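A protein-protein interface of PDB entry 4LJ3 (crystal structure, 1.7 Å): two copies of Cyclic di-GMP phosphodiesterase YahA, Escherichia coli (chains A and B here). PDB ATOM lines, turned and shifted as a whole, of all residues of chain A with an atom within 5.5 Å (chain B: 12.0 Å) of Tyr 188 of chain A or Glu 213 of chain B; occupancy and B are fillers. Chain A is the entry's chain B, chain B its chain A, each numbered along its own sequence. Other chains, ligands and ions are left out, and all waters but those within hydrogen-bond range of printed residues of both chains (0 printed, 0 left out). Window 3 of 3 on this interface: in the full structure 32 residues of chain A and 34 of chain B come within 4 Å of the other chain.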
ATOM      1  N   ALA A 186     -24.486  15.709 -15.746  1.00  0.00           N
ATOM      2  CA  ALA A 186     -24.277  15.060 -14.473  1.00  0.00           C
ATOM      3  C   ALA A 186     -23.058  14.125 -14.479  1.00  0.00           C
ATOM      4  O   ALA A 186     -23.176  12.900 -14.449  1.00  0.00           O
ATOM      5  CB  ALA A 186     -25.548  14.340 -13.976  1.00  0.00           C
ATOM      6  N   THR A 187     -21.877  14.742 -14.473  1.00  0.00           N
ATOM      7  CA  THR A 187     -20.638  14.074 -14.811  1.00  0.00           C
ATOM      8  C   THR A 187     -20.118  13.167 -13.719  1.00  0.00           C
ATOM      9  O   THR A 187     -19.648  12.077 -13.998  1.00  0.00           O
ATOM     10  CB  THR A 187     -19.574  15.093 -15.260  1.00  0.00           C
ATOM     11  OG1 THR A 187     -20.121  15.863 -16.348  1.00  0.00           O
ATOM     12  CG2 THR A 187     -18.287  14.399 -15.720  1.00  0.00           C
ATOM     13  N   TYR A 188     -20.257  13.606 -12.492  1.00  0.00           N
ATOM     14  CA  TYR A 188     -19.937  12.767 -11.363  1.00  0.00           C
ATOM     15  C   TYR A 188     -20.793  11.491 -11.376  1.00  0.00           C
ATOM     16  O   TYR A 188     -20.262  10.388 -11.288  1.00  0.00           O
ATOM     17  CB  TYR A 188     -20.067  13.567 -10.081  1.00  0.00           C
ATOM     18  CG  TYR A 188     -19.428  12.860  -8.906  1.00  0.00           C
ATOM     19  CD1 TYR A 188     -18.060  12.944  -8.710  1.00  0.00           C
ATOM     20  CD2 TYR A 188     -20.184  12.099  -8.027  1.00  0.00           C
ATOM     21  CE1 TYR A 188     -17.444  12.310  -7.643  1.00  0.00           C
ATOM     22  CE2 TYR A 188     -19.586  11.462  -6.938  1.00  0.00           C
ATOM     23  CZ  TYR A 188     -18.213  11.567  -6.762  1.00  0.00           C
ATOM     24  OH  TYR A 188     -17.556  10.941  -5.716  1.00  0.00           O
ATOM     25  N   ARG A 189     -22.110  11.639 -11.533  1.00  0.00           N
ATOM     26  CA  ARG A 189     -23.020  10.485 -11.640  1.00  0.00           C
ATOM     27  C   ARG A 189     -22.587   9.561 -12.766  1.00  0.00           C
ATOM     28  O   ARG A 189     -22.566   8.341 -12.602  1.00  0.00           O
ATOM     29  CB  ARG A 189     -24.473  10.924 -11.875  1.00  0.00           C
ATOM     30  CG  ARG A 189     -25.431   9.791 -12.251  1.00  0.00           C
ATOM     31  CD  ARG A 189     -26.882  10.227 -12.182  1.00  0.00           C
ATOM     32  NE  ARG A 189     -27.757   9.373 -12.995  1.00  0.00           N
ATOM     33  CZ  ARG A 189     -28.118   9.669 -14.238  1.00  0.00           C
ATOM     34  NH1 ARG A 189     -27.713  10.801 -14.795  1.00  0.00           N
ATOM     35  NH2 ARG A 189     -28.932   8.850 -14.916  1.00  0.00           N
ATOM     36  N   TYR A 190     -22.244  10.147 -13.905  1.00  0.00           N
ATOM     37  CA  TYR A 190     -21.835   9.363 -15.078  1.00  0.00           C
ATOM     38  C   TYR A 190     -20.581   8.537 -14.768  1.00  0.00           C
ATOM     39  O   TYR A 190     -20.515   7.336 -15.045  1.00  0.00           O
ATOM     40  CB  TYR A 190     -21.571  10.269 -16.283  1.00  0.00           C
ATOM     41  CG  TYR A 190     -21.223   9.472 -17.500  1.00  0.00           C
ATOM     42  CD1 TYR A 190     -22.201   9.093 -18.403  1.00  0.00           C
ATOM     43  CD2 TYR A 190     -19.894   9.079 -17.743  1.00  0.00           C
ATOM     44  CE1 TYR A 190     -21.870   8.360 -19.528  1.00  0.00           C
ATOM     45  CE2 TYR A 190     -19.559   8.344 -18.865  1.00  0.00           C
ATOM     46  CZ  TYR A 190     -20.562   8.000 -19.755  1.00  0.00           C
ATOM     47  OH  TYR A 190     -20.265   7.253 -20.887  1.00  0.00           O
ATOM     48  N   LEU A 191     -19.587   9.193 -14.167  1.00  0.00           N
ATOM     49  CA  LEU A 191     -18.332   8.493 -13.849  1.00  0.00           C
ATOM     50  C   LEU A 191     -18.529   7.424 -12.768  1.00  0.00           C
ATOM     51  O   LEU A 191     -17.814   6.429 -12.738  1.00  0.00           O
ATOM     52  CB  LEU A 191     -17.282   9.507 -13.385  1.00  0.00           C
ATOM     53  CG  LEU A 191     -16.767  10.405 -14.509  1.00  0.00           C
ATOM     54  CD1 LEU A 191     -15.894  11.519 -13.938  1.00  0.00           C
ATOM     55  CD2 LEU A 191     -16.004   9.570 -15.529  1.00  0.00           C
ATOM     56  N   GLN A 192     -19.478   7.643 -11.864  1.00  0.00           N
ATOM     57  CA  GLN A 192     -19.780   6.618 -10.865  1.00  0.00           C
ATOM     58  C   GLN A 192     -20.344   5.351 -11.509  1.00  0.00           C
ATOM     59  O   GLN A 192     -20.028   4.238 -11.097  1.00  0.00           O
ATOM     60  CB  GLN A 192     -20.732   7.161  -9.808  1.00  0.00           C
ATOM     61  CG  GLN A 192     -20.862   6.274  -8.600  1.00  0.00           C
ATOM     62  CD  GLN A 192     -21.533   6.989  -7.443  1.00  0.00           C
ATOM     63  OE1 GLN A 192     -21.016   7.981  -6.907  1.00  0.00           O
ATOM     64  NE2 GLN A 192     -22.694   6.503  -7.061  1.00  0.00           N
ATOM     65  N   ALA A 193     -21.168   5.528 -12.536  1.00  0.00           N
ATOM     66  CA  ALA A 193     -21.752   4.398 -13.275  1.00  0.00           C
ATOM     67  C   ALA A 193     -20.730   3.759 -14.208  1.00  0.00           C
ATOM     68  O   ALA A 193     -20.727   2.520 -14.402  1.00  0.00           O
ATOM     69  CB  ALA A 193     -22.941   4.886 -14.099  1.00  0.00           C
ATOM     70  N   LEU A 225     -11.661  20.225 -11.487  1.00  0.00           N
ATOM     71  CA  LEU A 225     -12.697  19.187 -11.426  1.00  0.00           C
ATOM     72  C   LEU A 225     -12.272  17.906 -12.147  1.00  0.00           C
ATOM     73  O   LEU A 225     -12.671  16.808 -11.761  1.00  0.00           O
ATOM     74  CB  LEU A 225     -13.999  19.693 -12.027  1.00  0.00           C
ATOM     75  CG  LEU A 225     -14.658  20.797 -11.206  1.00  0.00           C
ATOM     76  CD1 LEU A 225     -15.787  21.391 -12.015  1.00  0.00           C
ATOM     77  CD2 LEU A 225     -15.149  20.258  -9.848  1.00  0.00           C
ATOM     78  N   GLN B 207     -28.374  23.349 -18.238  1.00  0.00           N
ATOM     79  CA  GLN B 207     -28.927  22.004 -18.009  1.00  0.00           C
ATOM     80  C   GLN B 207     -28.183  21.150 -17.012  1.00  0.00           C
ATOM     81  O   GLN B 207     -28.590  20.009 -16.774  1.00  0.00           O
ATOM     82  CB  GLN B 207     -29.026  21.270 -19.344  1.00  0.00           C
ATOM     83  CG  GLN B 207     -29.961  21.976 -20.312  1.00  0.00           C
ATOM     84  CD  GLN B 207     -29.998  21.340 -21.679  1.00  0.00           C
ATOM     85  OE1 GLN B 207     -29.247  20.393 -21.955  1.00  0.00           O
ATOM     86  NE2 GLN B 207     -30.891  21.846 -22.552  1.00  0.00           N
ATOM     87  N   MET B 208     -27.101  21.674 -16.422  1.00  0.00           N
ATOM     88  CA  MET B 208     -26.338  20.912 -15.411  1.00  0.00           C
ATOM     89  C   MET B 208     -27.048  20.743 -14.064  1.00  0.00           C
ATOM     90  O   MET B 208     -27.599  21.689 -13.537  1.00  0.00           O
ATOM     91  CB  MET B 208     -24.965  21.549 -15.188  1.00  0.00           C
ATOM     92  CG  MET B 208     -24.045  21.327 -16.371  1.00  0.00           C
ATOM     93  SD  MET B 208     -22.456  22.144 -16.267  1.00  0.00           S
ATOM     94  CE  MET B 208     -21.729  21.643 -17.827  1.00  0.00           C
ATOM     95  N   ALA B 209     -26.976  19.535 -13.534  1.00  0.00           N
ATOM     96  CA  ALA B 209     -27.552  19.183 -12.216  1.00  0.00           C
ATOM     97  C   ALA B 209     -26.814  19.854 -11.056  1.00  0.00           C
ATOM     98  O   ALA B 209     -25.628  19.611 -10.844  1.00  0.00           O
ATOM     99  CB  ALA B 209     -27.557  17.679 -12.050  1.00  0.00           C
ATOM    100  N   SER B 210     -27.532  20.682 -10.278  1.00  0.00           N
ATOM    101  CA  SER B 210     -26.922  21.355  -9.112  1.00  0.00           C
ATOM    102  C   SER B 210     -26.283  20.413  -8.140  1.00  0.00           C
ATOM    103  O   SER B 210     -25.232  20.705  -7.547  1.00  0.00           O
ATOM    104  CB  SER B 210     -27.971  22.166  -8.342  1.00  0.00           C
ATOM    105  OG  SER B 210     -27.303  22.760  -7.244  1.00  0.00           O
ATOM    106  N   VAL B 211     -26.888  19.261  -7.938  1.00  0.00           N
ATOM    107  CA  VAL B 211     -26.361  18.328  -6.920  1.00  0.00           C
ATOM    108  C   VAL B 211     -25.123  17.569  -7.374  1.00  0.00           C
ATOM    109  O   VAL B 211     -24.412  16.987  -6.557  1.00  0.00           O
ATOM    110  CB  VAL B 211     -27.431  17.352  -6.425  1.00  0.00           C
ATOM    111  CG1 VAL B 211     -28.555  18.132  -5.769  1.00  0.00           C
ATOM    112  CG2 VAL B 211     -27.924  16.449  -7.561  1.00  0.00           C
ATOM    113  N   ASP B 212     -24.848  17.583  -8.676  1.00  0.00           N
ATOM    114  CA  ASP B 212     -23.713  16.837  -9.199  1.00  0.00           C
ATOM    115  C   ASP B 212     -22.395  17.425  -8.746  1.00  0.00           C
ATOM    116  O   ASP B 212     -22.137  18.616  -8.910  1.00  0.00           O
ATOM    117  CB  ASP B 212     -23.750  16.705 -10.724  1.00  0.00           C
ATOM    118  CG  ASP B 212     -22.805  15.622 -11.229  1.00  0.00           C
ATOM    119  OD1 ASP B 212     -23.184  14.439 -11.227  1.00  0.00           O
ATOM    120  OD2 ASP B 212     -21.678  15.972 -11.624  1.00  0.00           O
ATOM    121  N   GLU B 213     -21.571  16.561  -8.177  1.00  0.00           N
ATOM    122  CA  GLU B 213     -20.298  16.945  -7.591  1.00  0.00           C
ATOM    123  C   GLU B 213     -19.279  17.473  -8.608  1.00  0.00           C
ATOM    124  O   GLU B 213     -18.272  18.057  -8.219  1.00  0.00           O
ATOM    125  CB  GLU B 213     -19.733  15.777  -6.785  1.00  0.00           C
ATOM    126  CG  GLU B 213     -20.552  15.458  -5.515  1.00  0.00           C
ATOM    127  CD  GLU B 213     -21.664  14.394  -5.645  1.00  0.00           C
ATOM    128  OE1 GLU B 213     -22.240  14.253  -6.737  1.00  0.00           O
ATOM    129  OE2 GLU B 213     -21.991  13.695  -4.624  1.00  0.00           O
ATOM    130  N   ILE B 214     -19.535  17.277  -9.899  1.00  0.00           N
ATOM    131  CA  ILE B 214     -18.765  17.974 -10.919  1.00  0.00           C
ATOM    132  C   ILE B 214     -19.626  19.046 -11.579  1.00  0.00           C
ATOM    133  O   ILE B 214     -19.281  20.247 -11.524  1.00  0.00           O
ATOM    134  CB  ILE B 214     -18.170  16.982 -11.947  1.00  0.00           C
ATOM    135  CG1 ILE B 214     -17.080  16.171 -11.240  1.00  0.00           C
ATOM    136  CG2 ILE B 214     -17.674  17.714 -13.194  1.00  0.00           C
ATOM    137  CD1 ILE B 214     -16.529  15.015 -12.021  1.00  0.00           C
ATOM    138  N   SER B 215     -20.737  18.641 -12.206  1.00  0.00           N
ATOM    139  CA  SER B 215     -21.475  19.559 -13.074  1.00  0.00           C
ATOM    140  C   SER B 215     -22.114  20.709 -12.289  1.00  0.00           C
ATOM    141  O   SER B 215     -22.264  21.819 -12.835  1.00  0.00           O
ATOM    142  CB  SER B 215     -22.510  18.824 -13.922  1.00  0.00           C
ATOM    143  OG  SER B 215     -21.940  17.707 -14.609  1.00  0.00           O
ATOM    144  N   GLY B 216     -22.475  20.468 -11.021  1.00  0.00           N
ATOM    145  CA  GLY B 216     -23.073  21.529 -10.201  1.00  0.00           C
ATOM    146  C   GLY B 216     -22.074  22.630  -9.903  1.00  0.00           C
ATOM    147  O   GLY B 216     -22.461  23.788  -9.786  1.00  0.00           O
ATOM    148  N   HIS B 217     -20.788  22.268  -9.765  1.00  0.00           N
ATOM    149  CA  HIS B 217     -19.746  23.267  -9.569  1.00  0.00           C
ATOM    150  C   HIS B 217     -19.461  24.057 -10.824  1.00  0.00           C
ATOM    151  O   HIS B 217     -19.159  25.251 -10.740  1.00  0.00           O
ATOM    152  CB  HIS B 217     -18.467  22.649  -9.058  1.00  0.00           C
ATOM    153  CG  HIS B 217     -18.645  22.016  -7.738  1.00  0.00           C
ATOM    154  ND1 HIS B 217     -19.107  22.718  -6.647  1.00  0.00           N
ATOM    155  CD2 HIS B 217     -18.466  20.747  -7.324  1.00  0.00           C
ATOM    156  CE1 HIS B 217     -19.192  21.908  -5.610  1.00  0.00           C
ATOM    157  NE2 HIS B 217     -18.810  20.703  -5.991  1.00  0.00           N
ATOM    158  N   ILE B 218     -19.569  23.411 -11.984  1.00  0.00           N
ATOM    159  CA  ILE B 218     -19.385  24.123 -13.247  1.00  0.00           C
ATOM    160  C   ILE B 218     -20.449  25.184 -13.445  1.00  0.00           C
ATOM    161  O   ILE B 218     -20.113  26.353 -13.636  1.00  0.00           O
ATOM    162  CB  ILE B 218     -19.355  23.171 -14.475  1.00  0.00           C
ATOM    163  CG1 ILE B 218     -18.249  22.118 -14.305  1.00  0.00           C
ATOM    164  CG2 ILE B 218     -19.237  24.013 -15.754  1.00  0.00           C
ATOM    165  CD1 ILE B 218     -18.184  21.039 -15.375  1.00  0.00           C
ATOM    166  N   VAL B 219     -21.727  24.814 -13.393  1.00  0.00           N
ATOM    167  CA  VAL B 219     -22.769  25.794 -13.580  1.00  0.00           C
ATOM    168  C   VAL B 219     -22.721  26.889 -12.510  1.00  0.00           C
ATOM    169  O   VAL B 219     -22.933  28.061 -12.821  1.00  0.00           O
ATOM    170  CB  VAL B 219     -24.192  25.171 -13.700  1.00  0.00           C
ATOM    171  CG1 VAL B 219     -24.608  24.415 -12.462  1.00  0.00           C
ATOM    172  CG2 VAL B 219     -25.228  26.245 -14.038  1.00  0.00           C
ATOM    173  N   ASP B 220     -22.395  26.516 -11.276  1.00  0.00           N
ATOM    174  CA  ASP B 220     -22.216  27.520 -10.215  1.00  0.00           C
ATOM    175  C   ASP B 220     -21.208  28.591 -10.635  1.00  0.00           C
ATOM    176  O   ASP B 220     -21.443  29.790 -10.489  1.00  0.00           O
ATOM    177  CB  ASP B 220     -21.721  26.857  -8.929  1.00  0.00           C
ATOM    178  CG  ASP B 220     -22.841  26.230  -8.118  1.00  0.00           C
ATOM    179  OD1 ASP B 220     -24.012  26.352  -8.541  1.00  0.00           O
ATOM    180  OD2 ASP B 220     -22.564  25.596  -7.057  1.00  0.00           O
ATOM    181  N   ASN B 221     -20.072  28.134 -11.125  1.00  0.00           N
ATOM    182  CA  ASN B 221     -18.978  28.984 -11.510  1.00  0.00           C
ATOM    183  C   ASN B 221     -19.351  29.872 -12.684  1.00  0.00           C
ATOM    184  O   ASN B 221     -19.104  31.078 -12.661  1.00  0.00           O
ATOM    185  CB  ASN B 221     -17.749  28.138 -11.840  1.00  0.00           C
ATOM    186  CG  ASN B 221     -16.519  28.982 -12.032  1.00  0.00           C
ATOM    187  OD1 ASN B 221     -16.173  29.782 -11.143  1.00  0.00           O
ATOM    188  ND2 ASN B 221     -15.868  28.844 -13.177  1.00  0.00           N
ATOM    189  N   LEU B 246     -33.308  25.957 -10.567  1.00  0.00           N
ATOM    190  CA  LEU B 246     -31.910  26.309 -10.274  1.00  0.00           C
ATOM    191  C   LEU B 246     -31.612  27.729 -10.751  1.00  0.00           C
ATOM    192  O   LEU B 246     -30.997  28.533 -10.050  1.00  0.00           O
ATOM    193  CB  LEU B 246     -30.908  25.317 -10.880  1.00  0.00           C
ATOM    194  CG  LEU B 246     -29.434  25.587 -10.548  1.00  0.00           C
ATOM    195  CD1 LEU B 246     -29.186  25.418  -9.064  1.00  0.00           C
ATOM    196  CD2 LEU B 246     -28.497  24.710 -11.372  1.00  0.00           C
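Tyr 188 of chain A touches just these residues of chain B: Asp 212 (2.9 Å), Glu 213 (3.2 Å) and Ile 214 (3.8 Å).
Of chain A, only Tyr 188 comes within 4 Å of Glu 213 of chain B.
Printed residues of chain B within 4 Å of Ala 186 of chain A: Asp 212 (3.3 Å) and Ser 215 (3.4 Å).
Printed residues of chain B within 4 Å of Thr 187 of chain A: Asp 212, Ile 214 and Ser 215.
No residue of chain B comes within 4 Å of Gln 192 of chain A.
Of chain B, only Ile 214 (3.7 Å) and Ile 218 (3.4 Å) come within 4 Å of Leu 225 of chain A.
Printed residues of chain A within 4 Å of Ile 214 of chain B: Thr 187 (3.8 Å), Tyr 188 (3.8 Å) and Leu 225 (3.7 Å).
Of the printed residues of chain A, Ser 215 of chain B touches Ala 186 and Thr 187.
Tyr 190 of chain A touches none of the printed residues of chain B.
Leu 246 of chain B touches none of the printed residues of chain A.
Asp 212 of chain B touches Ala 186 of chain A (OD1 to C, 3.3 Å).
Ile 214 of chain B touches Thr 187 of chain A.
CD2 of Tyr 188 of chain A touches OE1 of Glu 213 of chain B, 3.2 Å away.
CB of Tyr 188 of chain A touches N of Ile 214 of chain B (3.8 Å).
Leu 225 of chain A touches Ile 214 of chain B.
Leu 225 of chain A touches Ile 218 of chain B (CD1 to CG1, 3.4 Å).
No position is printed for both chains.
Of the 11 pairs that touch across the chains among the printed residues, none has its exchanged pair printed and touching as well.
The side-chain carboxylate of Asp 212 of chain B is in hydrogen-bond range of the backbone NH of Ile 214 of chain B, 3.0 Å away.
The side-chain carboxylate (OD2) of Asp 212 of chain B is in hydrogen-bond range of the backbone NH (N) of Ser 215 of chain B.
The backbone NH (N) of Thr 187 of chain A sits at hydrogen-bond distance from the side-chain carboxylate (OD2) of Asp 212 of chain B, at 3.1 Å.
The backbone NH (N) of Tyr 188 of chain A sits at hydrogen-bond distance from the side-chain carboxylate (OD2) of Asp 212 of chain B (2.9 Å).
The backbone NH (N) of Arg 189 of chain A lies within hydrogen-bond range of the side-chain carboxylate (OD1) of Asp 212 of chain B (3.0 Å).
The side-chain hydroxyl of Ser 215 of chain B lies within hydrogen-bond range of the backbone NH of Ala 186 of chain A (3.4 Å).
OG of Ser 215 of chain B sits at hydrogen-bond distance from N of Thr 187 of chain A.
Of the 16 printed residues of chain B, 5 touch a printed residue of chain A.
Printed residues of chain B that touch a printed residue of chain A: Asp 212, Glu 213, Ile 214, Ser 215 and Ile 218.
Hydrophobic or aromatic side chains of chain B within 4 Å of the printed part of chain A: Ile 214 and Ile 218.
Printed residues of chain A that touch a printed residue of chain B: Ala 186, Thr 187, Tyr 188, Arg 189 and Leu 225.
Hydrophobic or aromatic side chains of chain A within 4 Å of the printed part of chain B: Ala 186, Tyr 188 and Leu 225.
Among the printed residues, 11 pairs touch across the chains.
Among the printed residues, no Asp or Glu carboxylate lies within 4 Å of a Lys or Arg side-chain nitrogen of the other chain.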
